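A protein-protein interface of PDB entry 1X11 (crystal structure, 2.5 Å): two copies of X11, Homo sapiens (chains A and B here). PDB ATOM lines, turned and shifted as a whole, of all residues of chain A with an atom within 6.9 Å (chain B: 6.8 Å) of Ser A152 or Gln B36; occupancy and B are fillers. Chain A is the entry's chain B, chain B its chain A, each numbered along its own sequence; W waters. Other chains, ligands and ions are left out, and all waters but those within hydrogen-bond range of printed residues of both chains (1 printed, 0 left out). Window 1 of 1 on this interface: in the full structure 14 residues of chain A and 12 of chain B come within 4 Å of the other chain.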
ATOM      1  N   ILE A   8      17.452 -24.314  16.285  1.00  0.00           N
ATOM      2  CA  ILE A   8      17.735 -25.644  15.698  1.00  0.00           C
ATOM      3  C   ILE A   8      16.440 -26.245  15.202  1.00  0.00           C
ATOM      4  O   ILE A   8      15.554 -26.534  15.992  1.00  0.00           O
ATOM      5  CB  ILE A   8      18.299 -26.619  16.722  1.00  0.00           C
ATOM      6  CG1 ILE A   8      19.636 -26.122  17.264  1.00  0.00           C
ATOM      7  CG2 ILE A   8      18.470 -27.994  16.076  1.00  0.00           C
ATOM      8  CD1 ILE A   8      20.294 -27.109  18.228  1.00  0.00           C
ATOM      9  N   ILE A   9      16.340 -26.444  13.897  1.00  0.00           N
ATOM     10  CA  ILE A   9      15.151 -27.008  13.295  1.00  0.00           C
ATOM     11  C   ILE A   9      15.577 -27.923  12.157  1.00  0.00           C
ATOM     12  O   ILE A   9      16.380 -27.545  11.307  1.00  0.00           O
ATOM     13  CB  ILE A   9      14.226 -25.901  12.755  1.00  0.00           C
ATOM     14  CG1 ILE A   9      13.910 -24.891  13.868  1.00  0.00           C
ATOM     15  CG2 ILE A   9      12.934 -26.517  12.232  1.00  0.00           C
ATOM     16  CD1 ILE A   9      13.550 -23.512  13.356  1.00  0.00           C
ATOM     17  N   PHE A  10      15.082 -29.146  12.185  1.00  0.00           N
ATOM     18  CA  PHE A  10      15.411 -30.101  11.149  1.00  0.00           C
ATOM     19  C   PHE A  10      14.130 -30.646  10.517  1.00  0.00           C
ATOM     20  O   PHE A  10      13.047 -30.551  11.106  1.00  0.00           O
ATOM     21  CB  PHE A  10      16.269 -31.222  11.735  1.00  0.00           C
ATOM     22  CG  PHE A  10      17.670 -30.787  12.067  1.00  0.00           C
ATOM     23  CD1 PHE A  10      18.508 -30.276  11.073  1.00  0.00           C
ATOM     24  CD2 PHE A  10      18.151 -30.869  13.379  1.00  0.00           C
ATOM     25  CE1 PHE A  10      19.803 -29.840  11.381  1.00  0.00           C
ATOM     26  CE2 PHE A  10      19.446 -30.433  13.696  1.00  0.00           C
ATOM     27  CZ  PHE A  10      20.271 -29.921  12.692  1.00  0.00           C
ATOM     28  N   ILE A  70      13.999 -27.792  17.855  1.00  0.00           N
ATOM     29  CA  ILE A  70      14.747 -28.250  19.028  1.00  0.00           C
ATOM     30  C   ILE A  70      15.375 -27.176  19.907  1.00  0.00           C
ATOM     31  O   ILE A  70      16.100 -26.312  19.422  1.00  0.00           O
ATOM     32  CB  ILE A  70      15.886 -29.189  18.573  1.00  0.00           C
ATOM     33  CG1 ILE A  70      15.324 -30.361  17.767  1.00  0.00           C
ATOM     34  CG2 ILE A  70      16.697 -29.650  19.766  1.00  0.00           C
ATOM     35  CD1 ILE A  70      16.205 -30.768  16.611  1.00  0.00           C
ATOM     36  N   LEU A  71      15.140 -27.266  21.209  1.00  0.00           N
ATOM     37  CA  LEU A  71      15.737 -26.320  22.138  1.00  0.00           C
ATOM     38  C   LEU A  71      15.881 -26.950  23.518  1.00  0.00           C
ATOM     39  O   LEU A  71      15.559 -28.124  23.707  1.00  0.00           O
ATOM     40  CB  LEU A  71      14.944 -25.017  22.225  1.00  0.00           C
ATOM     41  CG  LEU A  71      13.617 -25.012  22.970  1.00  0.00           C
ATOM     42  CD1 LEU A  71      13.075 -23.587  23.101  1.00  0.00           C
ATOM     43  CD2 LEU A  71      12.646 -25.893  22.225  1.00  0.00           C
ATOM     44  N   ILE A  75      10.598 -29.654  22.643  1.00  0.00           N
ATOM     45  CA  ILE A  75      10.766 -30.213  21.295  1.00  0.00           C
ATOM     46  C   ILE A  75       9.375 -30.101  20.673  1.00  0.00           C
ATOM     47  O   ILE A  75       8.413 -30.652  21.221  1.00  0.00           O
ATOM     48  CB  ILE A  75      11.182 -31.722  21.263  1.00  0.00           C
ATOM     49  CG1 ILE A  75      12.408 -31.984  22.129  1.00  0.00           C
ATOM     50  CG2 ILE A  75      11.496 -32.135  19.837  1.00  0.00           C
ATOM     51  CD1 ILE A  75      13.630 -31.218  21.740  1.00  0.00           C
ATOM     52  N   GLN A 147      20.684 -38.635  12.571  1.00  0.00           N
ATOM     53  CA  GLN A 147      21.725 -38.698  13.591  1.00  0.00           C
ATOM     54  C   GLN A 147      21.949 -37.316  14.199  1.00  0.00           C
ATOM     55  O   GLN A 147      22.156 -37.179  15.404  1.00  0.00           O
ATOM     56  CB  GLN A 147      23.012 -39.234  12.975  1.00  0.00           C
ATOM     57  CG  GLN A 147      24.285 -39.003  13.797  1.00  0.00           C
ATOM     58  CD  GLN A 147      24.396 -39.868  15.063  1.00  0.00           C
ATOM     59  OE1 GLN A 147      25.205 -40.802  15.101  1.00  0.00           O
ATOM     60  NE2 GLN A 147      23.649 -39.517  16.112  1.00  0.00           N
ATOM     61  N   LEU A 148      21.872 -36.288  13.363  1.00  0.00           N
ATOM     62  CA  LEU A 148      22.059 -34.907  13.804  1.00  0.00           C
ATOM     63  C   LEU A 148      20.875 -34.418  14.642  1.00  0.00           C
ATOM     64  O   LEU A 148      21.031 -33.541  15.482  1.00  0.00           O
ATOM     65  CB  LEU A 148      22.288 -34.003  12.588  1.00  0.00           C
ATOM     66  CG  LEU A 148      22.632 -32.524  12.738  1.00  0.00           C
ATOM     67  CD1 LEU A 148      23.712 -32.284  13.789  1.00  0.00           C
ATOM     68  CD2 LEU A 148      23.047 -31.997  11.374  1.00  0.00           C
ATOM     69  N   ILE A 149      19.697 -34.978  14.399  1.00  0.00           N
ATOM     70  CA  ILE A 149      18.497 -34.636  15.152  1.00  0.00           C
ATOM     71  C   ILE A 149      18.636 -35.243  16.555  1.00  0.00           C
ATOM     72  O   ILE A 149      18.345 -34.586  17.560  1.00  0.00           O
ATOM     73  CB  ILE A 149      17.235 -35.207  14.453  1.00  0.00           C
ATOM     74  CG1 ILE A 149      16.908 -34.397  13.207  1.00  0.00           C
ATOM     75  CG2 ILE A 149      16.045 -35.221  15.391  1.00  0.00           C
ATOM     76  CD1 ILE A 149      15.728 -34.923  12.486  1.00  0.00           C
ATOM     77  N   ALA A 150      19.072 -36.499  16.623  1.00  0.00           N
ATOM     78  CA  ALA A 150      19.279 -37.182  17.901  1.00  0.00           C
ATOM     79  C   ALA A 150      20.434 -36.494  18.665  1.00  0.00           C
ATOM     80  O   ALA A 150      20.286 -36.121  19.847  1.00  0.00           O
ATOM     81  CB  ALA A 150      19.580 -38.679  17.681  1.00  0.00           C
ATOM     82  N   GLN A 151      21.569 -36.309  17.984  1.00  0.00           N
ATOM     83  CA  GLN A 151      22.724 -35.641  18.581  1.00  0.00           C
ATOM     84  C   GLN A 151      22.277 -34.293  19.142  1.00  0.00           C
ATOM     85  O   GLN A 151      22.613 -33.964  20.276  1.00  0.00           O
ATOM     86  CB  GLN A 151      23.807 -35.372  17.546  1.00  0.00           C
ATOM     87  CG  GLN A 151      24.805 -36.478  17.285  1.00  0.00           C
ATOM     88  CD  GLN A 151      25.821 -36.051  16.213  1.00  0.00           C
ATOM     89  OE1 GLN A 151      26.295 -34.891  16.179  1.00  0.00           O
ATOM     90  NE2 GLN A 151      26.149 -36.979  15.325  1.00  0.00           N
ATOM     91  N   SER A 152      21.530 -33.525  18.343  1.00  0.00           N
ATOM     92  CA  SER A 152      21.026 -32.215  18.762  1.00  0.00           C
ATOM     93  C   SER A 152      20.106 -32.293  19.969  1.00  0.00           C
ATOM     94  O   SER A 152      20.211 -31.461  20.883  1.00  0.00           O
ATOM     95  CB  SER A 152      20.286 -31.506  17.630  1.00  0.00           C
ATOM     96  OG  SER A 152      21.157 -31.214  16.571  1.00  0.00           O
ATOM     97  N   ILE A 153      19.202 -33.271  19.979  1.00  0.00           N
ATOM     98  CA  ILE A 153      18.299 -33.414  21.103  1.00  0.00           C
ATOM     99  C   ILE A 153      19.033 -33.873  22.353  1.00  0.00           C
ATOM    100  O   ILE A 153      18.700 -33.456  23.455  1.00  0.00           O
ATOM    101  CB  ILE A 153      17.145 -34.337  20.784  1.00  0.00           C
ATOM    102  CG1 ILE A 153      16.298 -33.708  19.677  1.00  0.00           C
ATOM    103  CG2 ILE A 153      16.323 -34.567  22.029  1.00  0.00           C
ATOM    104  CD1 ILE A 153      15.020 -34.443  19.417  1.00  0.00           C
ATOM    105  N   GLY A 154      20.055 -34.705  22.180  1.00  0.00           N
ATOM    106  CA  GLY A 154      20.843 -35.141  23.326  1.00  0.00           C
ATOM    107  C   GLY A 154      21.632 -33.959  23.895  1.00  0.00           C
ATOM    108  O   GLY A 154      21.794 -33.830  25.099  1.00  0.00           O
ATOM    109  N   GLN A 155      22.138 -33.098  23.016  1.00  0.00           N
ATOM    110  CA  GLN A 155      22.889 -31.928  23.440  1.00  0.00           C
ATOM    111  C   GLN A 155      21.930 -31.051  24.210  1.00  0.00           C
ATOM    112  O   GLN A 155      22.244 -30.581  25.314  1.00  0.00           O
ATOM    113  CB  GLN A 155      23.475 -31.177  22.240  1.00  0.00           C
ATOM    114  CG  GLN A 155      24.678 -31.873  21.588  1.00  0.00           C
ATOM    115  CD  GLN A 155      25.897 -31.922  22.489  1.00  0.00           C
ATOM    116  OE1 GLN A 155      25.981 -31.197  23.476  1.00  0.00           O
ATOM    117  NE2 GLN A 155      26.838 -32.797  22.170  1.00  0.00           N
ATOM    118  N   ALA A 156      20.732 -30.885  23.660  1.00  0.00           N
ATOM    119  CA  ALA A 156      19.706 -30.090  24.329  1.00  0.00           C
ATOM    120  C   ALA A 156      19.544 -30.642  25.751  1.00  0.00           C
ATOM    121  O   ALA A 156      19.569 -29.878  26.726  1.00  0.00           O
ATOM    122  CB  ALA A 156      18.372 -30.128  23.553  1.00  0.00           C
ATOM    123  N   PHE A 157      19.469 -31.970  25.867  1.00  0.00           N
ATOM    124  CA  PHE A 157      19.344 -32.623  27.164  1.00  0.00           C
ATOM    125  C   PHE A 157      20.456 -32.118  28.070  1.00  0.00           C
ATOM    126  O   PHE A 157      20.165 -31.513  29.100  1.00  0.00           O
ATOM    127  CB  PHE A 157      19.449 -34.150  27.045  1.00  0.00           C
ATOM    128  CG  PHE A 157      18.226 -34.814  26.472  1.00  0.00           C
ATOM    129  CD1 PHE A 157      16.995 -34.174  26.461  1.00  0.00           C
ATOM    130  CD2 PHE A 157      18.309 -36.098  25.962  1.00  0.00           C
ATOM    131  CE1 PHE A 157      15.864 -34.802  25.937  1.00  0.00           C
ATOM    132  CE2 PHE A 157      17.183 -36.739  25.431  1.00  0.00           C
ATOM    133  CZ  PHE A 157      15.958 -36.088  25.427  1.00  0.00           C
ATOM    134  N   ASN B  29      28.768 -27.999  25.560  1.00  0.00           N
ATOM    135  CA  ASN B  29      27.466 -28.478  25.139  1.00  0.00           C
ATOM    136  C   ASN B  29      26.712 -27.409  24.369  1.00  0.00           C
ATOM    137  O   ASN B  29      26.123 -27.678  23.315  1.00  0.00           O
ATOM    138  CB  ASN B  29      26.687 -28.900  26.361  1.00  0.00           C
ATOM    139  CG  ASN B  29      27.321 -30.070  27.056  1.00  0.00           C
ATOM    140  OD1 ASN B  29      27.883 -29.923  28.141  1.00  0.00           O
ATOM    141  ND2 ASN B  29      27.257 -31.245  26.427  1.00  0.00           N
ATOM    142  N   VAL B  30      26.711 -26.195  24.914  1.00  0.00           N
ATOM    143  CA  VAL B  30      26.062 -25.054  24.266  1.00  0.00           C
ATOM    144  C   VAL B  30      26.845 -24.718  22.992  1.00  0.00           C
ATOM    145  O   VAL B  30      26.278 -24.273  22.001  1.00  0.00           O
ATOM    146  CB  VAL B  30      26.053 -23.849  25.202  1.00  0.00           C
ATOM    147  CG1 VAL B  30      25.686 -22.602  24.439  1.00  0.00           C
ATOM    148  CG2 VAL B  30      25.077 -24.093  26.341  1.00  0.00           C
ATOM    149  N   ARG B  31      28.162 -24.918  23.044  1.00  0.00           N
ATOM    150  CA  ARG B  31      29.044 -24.690  21.906  1.00  0.00           C
ATOM    151  C   ARG B  31      28.610 -25.649  20.823  1.00  0.00           C
ATOM    152  O   ARG B  31      28.391 -25.248  19.686  1.00  0.00           O
ATOM    153  CB  ARG B  31      30.498 -24.969  22.282  1.00  0.00           C
ATOM    154  CG  ARG B  31      31.185 -23.855  23.065  1.00  0.00           C
ATOM    155  CD  ARG B  31      31.971 -22.925  22.154  1.00  0.00           C
ATOM    156  NE  ARG B  31      31.281 -21.683  21.829  1.00  0.00           N
ATOM    157  CZ  ARG B  31      31.813 -20.477  22.005  1.00  0.00           C
ATOM    158  NH1 ARG B  31      33.035 -20.351  22.509  1.00  0.00           N
ATOM    159  NH2 ARG B  31      31.135 -19.396  21.655  1.00  0.00           N
ATOM    160  N   MET B  32      28.466 -26.919  21.173  1.00  0.00           N
ATOM    161  CA  MET B  32      28.020 -27.895  20.200  1.00  0.00           C
ATOM    162  C   MET B  32      26.583 -27.597  19.750  1.00  0.00           C
ATOM    163  O   MET B  32      26.257 -27.786  18.578  1.00  0.00           O
ATOM    164  CB  MET B  32      28.148 -29.315  20.729  1.00  0.00           C
ATOM    165  CG  MET B  32      27.847 -30.376  19.669  1.00  0.00           C
ATOM    166  SD  MET B  32      28.888 -30.289  18.167  1.00  0.00           S
ATOM    167  CE  MET B  32      30.534 -30.560  18.922  1.00  0.00           C
ATOM    168  N   MET B  33      25.741 -27.081  20.652  1.00  0.00           N
ATOM    169  CA  MET B  33      24.361 -26.737  20.287  1.00  0.00           C
ATOM    170  C   MET B  33      24.354 -25.580  19.284  1.00  0.00           C
ATOM    171  O   MET B  33      23.528 -25.558  18.374  1.00  0.00           O
ATOM    172  CB  MET B  33      23.542 -26.347  21.513  1.00  0.00           C
ATOM    173  CG  MET B  33      22.792 -27.471  22.187  1.00  0.00           C
ATOM    174  SD  MET B  33      21.489 -26.822  23.268  1.00  0.00           S
ATOM    175  CE  MET B  33      20.057 -26.975  22.169  1.00  0.00           C
ATOM    176  N   GLN B  34      25.298 -24.647  19.444  1.00  0.00           N
ATOM    177  CA  GLN B  34      25.472 -23.464  18.574  1.00  0.00           C
ATOM    178  C   GLN B  34      25.953 -23.858  17.184  1.00  0.00           C
ATOM    179  O   GLN B  34      25.527 -23.277  16.173  1.00  0.00           O
ATOM    180  CB  GLN B  34      26.491 -22.478  19.160  1.00  0.00           C
ATOM    181  CG  GLN B  34      26.101 -21.890  20.486  1.00  0.00           C
ATOM    182  CD  GLN B  34      27.062 -20.825  20.937  1.00  0.00           C
ATOM    183  OE1 GLN B  34      28.077 -20.578  20.296  1.00  0.00           O
ATOM    184  NE2 GLN B  34      26.757 -20.186  22.050  1.00  0.00           N
ATOM    185  N   ALA B  35      26.908 -24.788  17.161  1.00  0.00           N
ATOM    186  CA  ALA B  35      27.464 -25.311  15.926  1.00  0.00           C
ATOM    187  C   ALA B  35      26.322 -26.041  15.201  1.00  0.00           C
ATOM    188  O   ALA B  35      26.073 -25.819  14.007  1.00  0.00           O
ATOM    189  CB  ALA B  35      28.611 -26.259  16.245  1.00  0.00           C
ATOM    190  N   GLN B  36      25.577 -26.834  15.969  1.00  0.00           N
ATOM    191  CA  GLN B  36      24.431 -27.602  15.472  1.00  0.00           C
ATOM    192  C   GLN B  36      23.384 -26.680  14.867  1.00  0.00           C
ATOM    193  O   GLN B  36      22.845 -26.935  13.781  1.00  0.00           O
ATOM    194  CB  GLN B  36      23.808 -28.407  16.622  1.00  0.00           C
ATOM    195  CG  GLN B  36      24.645 -29.617  17.036  1.00  0.00           C
ATOM    196  CD  GLN B  36      24.151 -30.304  18.303  1.00  0.00           C
ATOM    197  OE1 GLN B  36      24.463 -31.485  18.545  1.00  0.00           O
ATOM    198  NE2 GLN B  36      23.393 -29.575  19.128  1.00  0.00           N
ATOM    199  N   GLU B  37      23.114 -25.597  15.587  1.00  0.00           N
ATOM    200  CA  GLU B  37      22.153 -24.586  15.167  1.00  0.00           C
ATOM    201  C   GLU B  37      22.629 -23.979  13.851  1.00  0.00           C
ATOM    202  O   GLU B  37      21.821 -23.714  12.964  1.00  0.00           O
ATOM    203  CB  GLU B  37      22.039 -23.519  16.251  1.00  0.00           C
ATOM    204  CG  GLU B  37      20.958 -22.503  16.055  1.00  0.00           C
ATOM    205  CD  GLU B  37      20.735 -21.665  17.313  1.00  0.00           C
ATOM    206  OE1 GLU B  37      20.906 -22.210  18.434  1.00  0.00           O
ATOM    207  OE2 GLU B  37      20.382 -20.469  17.170  1.00  0.00           O
ATOM    208  N   ALA B  38      23.950 -23.831  13.715  1.00  0.00           N
ATOM    209  CA  ALA B  38      24.573 -23.279  12.514  1.00  0.00           C
ATOM    210  C   ALA B  38      24.258 -24.151  11.320  1.00  0.00           C
ATOM    211  O   ALA B  38      23.768 -23.672  10.297  1.00  0.00           O
ATOM    212  CB  ALA B  38      26.068 -23.191  12.694  1.00  0.00           C
ATOM    213  N   VAL B  39      24.538 -25.441  11.449  1.00  0.00           N
ATOM    214  CA  VAL B  39      24.277 -26.377  10.362  1.00  0.00           C
ATOM    215  C   VAL B  39      22.811 -26.278   9.958  1.00  0.00           C
ATOM    216  O   VAL B  39      22.491 -26.095   8.788  1.00  0.00           O
ATOM    217  CB  VAL B  39      24.570 -27.835  10.771  1.00  0.00           C
ATOM    218  CG1 VAL B  39      24.403 -28.754   9.572  1.00  0.00           C
ATOM    219  CG2 VAL B  39      25.985 -27.958  11.343  1.00  0.00           C
ATOM    220  N   SER B  40      21.933 -26.373  10.951  1.00  0.00           N
ATOM    221  CA  SER B  40      20.494 -26.303  10.728  1.00  0.00           C
ATOM    222  C   SER B  40      20.122 -25.099   9.866  1.00  0.00           C
ATOM    223  O   SER B  40      19.420 -25.249   8.856  1.00  0.00           O
ATOM    224  CB  SER B  40      19.756 -26.255  12.070  1.00  0.00           C
ATOM    225  OG  SER B  40      18.409 -25.839  11.899  1.00  0.00           O
ATOM    226  N   ARG B  41      20.624 -23.923  10.244  1.00  0.00           N
ATOM    227  CA  ARG B  41      20.332 -22.708   9.504  1.00  0.00           C
ATOM    228  C   ARG B  41      20.816 -22.858   8.084  1.00  0.00           C
ATOM    229  O   ARG B  41      20.174 -22.374   7.144  1.00  0.00           O
ATOM    230  CB  ARG B  41      21.014 -21.494  10.111  1.00  0.00           C
ATOM    231  CG  ARG B  41      20.422 -21.004  11.385  1.00  0.00           C
ATOM    232  CD  ARG B  41      20.881 -19.581  11.599  1.00  0.00           C
ATOM    233  NE  ARG B  41      20.701 -19.115  12.972  1.00  0.00           N
ATOM    234  CZ  ARG B  41      21.013 -17.891  13.389  1.00  0.00           C
ATOM    235  NH1 ARG B  41      21.516 -17.001  12.531  1.00  0.00           N
ATOM    236  NH2 ARG B  41      20.834 -17.567  14.671  1.00  0.00           N
ATOM    237  N   LYS B  43      21.320 -25.825   6.299  1.00  0.00           N
ATOM    238  CA  LYS B  43      20.519 -26.807   5.571  1.00  0.00           C
ATOM    239  C   LYS B  43      19.186 -26.227   5.117  1.00  0.00           C
ATOM    240  O   LYS B  43      18.854 -26.251   3.935  1.00  0.00           O
ATOM    241  CB  LYS B  43      20.229 -28.035   6.438  1.00  0.00           C
ATOM    242  CG  LYS B  43      21.413 -28.903   6.863  1.00  0.00           C
ATOM    243  CD  LYS B  43      20.872 -30.059   7.714  1.00  0.00           C
ATOM    244  CE  LYS B  43      21.943 -30.844   8.453  1.00  0.00           C
ATOM    245  NZ  LYS B  43      22.796 -31.651   7.537  1.00  0.00           N
ATOM    246  N   ILE B 100      30.879 -32.229  12.785  1.00  0.00           N
ATOM    247  CA  ILE B 100      29.636 -32.970  12.924  1.00  0.00           C
ATOM    248  C   ILE B 100      29.536 -33.842  11.681  1.00  0.00           C
ATOM    249  O   ILE B 100      28.979 -33.443  10.648  1.00  0.00           O
ATOM    250  CB  ILE B 100      28.420 -32.059  13.078  1.00  0.00           C
ATOM    251  CG1 ILE B 100      28.786 -30.852  13.950  1.00  0.00           C
ATOM    252  CG2 ILE B 100      27.339 -32.833  13.769  1.00  0.00           C
ATOM    253  CD1 ILE B 100      27.612 -30.059  14.446  1.00  0.00           C
ATOM    254  N   VAL B 105      32.442 -26.699  11.403  1.00  0.00           N
ATOM    255  CA  VAL B 105      31.925 -25.387  11.789  1.00  0.00           C
ATOM    256  C   VAL B 105      32.996 -24.534  12.465  1.00  0.00           C
ATOM    257  O   VAL B 105      33.503 -24.867  13.540  1.00  0.00           O
ATOM    258  CB  VAL B 105      30.688 -25.463  12.683  1.00  0.00           C
ATOM    259  CG1 VAL B 105      30.236 -24.023  13.089  1.00  0.00           C
ATOM    260  CG2 VAL B 105      29.572 -26.216  11.948  1.00  0.00           C
ATOM    261  N   MET B 107      33.834 -21.059  14.115  1.00  0.00           N
ATOM    262  CA  MET B 107      33.146 -19.975  14.808  1.00  0.00           C
ATOM    263  C   MET B 107      34.054 -18.792  15.159  1.00  0.00           C
ATOM    264  O   MET B 107      34.875 -18.905  16.064  1.00  0.00           O
ATOM    265  CB  MET B 107      32.495 -20.541  16.070  1.00  0.00           C
ATOM    266  CG  MET B 107      31.244 -19.818  16.539  1.00  0.00           C
ATOM    267  SD  MET B 107      30.480 -20.623  17.957  1.00  0.00           S
ATOM    268  CE  MET B 107      29.849 -22.092  17.222  1.00  0.00           C
HETATM  269  O   HOH W   1      17.632 -23.178  13.812  1.00  0.00           O
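The side-chain hydroxyl (OG) of Ser A152 sits at hydrogen-bond distance from the backbone carbonyl oxygen (O) of Leu A148, 2.6 Å away. The side-chain carboxylate of Glu B37 is in salt-bridge range of the guanidinium group of Arg B41, 3.9 Å away. O of Met B32 lies close to NE2 of Gln B36, 3.4 Å away. The backbone NH (N) of Ile A70 lies within hydrogen-bond range of the backbone carbonyl oxygen (O) of Ile A8, 2.7 Å away.
No position is printed for both chains. Of the 17 pairs that touch across the chains among the printed residues, none has its exchanged pair printed and touching as well.
Met B33 touches Ile A8 (O to CD1, 3.6 Å). Ser B40 touches Ile A8 (OG to CA, 3.9 Å). Ser B40 touches Phe A10 (CB to CE1, 3.7 Å). Lys B43 touches Phe A10. Leu A148 touches Ile B100 (CD1 to CG2, 3.7 Å). OE1 of Gln A151 touches CG2 of Ile B100, 3.3 Å away. Ser A152 touches Gln B36 (CA to OE1, 3.5 Å). CG of Met B32 touches NE2 of Gln A155 (3.6 Å). CG of Met B33 touches CB of Gln A155, 3.8 Å away. CG of Gln A155 touches OE1 of Gln B36, at 3.1 Å.
Of chain B, only Gln B36 comes within 4 Å of Ser A152. Of the printed residues of chain A, Gln B36 touches Gln A151 (3.5 Å), Ser A152 (3.5 Å) and Gln A155 (3.1 Å). Of the printed residues of chain A, Glu B37 touches Ile A8. Of the printed residues of chain A, Val B39 touches Leu A148 (3.95 Å). The nearest residue of chain B that does not touch Ser A152 is Met B33 (4.7 Å). The nearest printed residue of chain A that does not touch Val B39 is Phe A10 (4.9 Å).
Hydrophobic or aromatic side chains of chain B within 4 Å of the printed part of chain A: Met B32, Met B33, Val B39 and Ile B100. Hydrophobic or aromatic side chains of chain A that line the printed part of chain B: Ile A8, Phe A10, Leu A148 and Ala A156. Along chain A the printed residues that touch a printed residue of chain B span positions 8 to 156.
OG of Ser B40 is in hydrogen-bond range of O of Ile A9, 2.7 Å away. The side-chain amide nitrogen (ND2) of Asn B29 sits at hydrogen-bond distance from the side-chain amide oxygen (OE1) of Gln A155, 3.2 Å away.
Water W1 bridges N of Ile A8 (2.7 Å) and OG of Ser B40 (3.4 Å).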
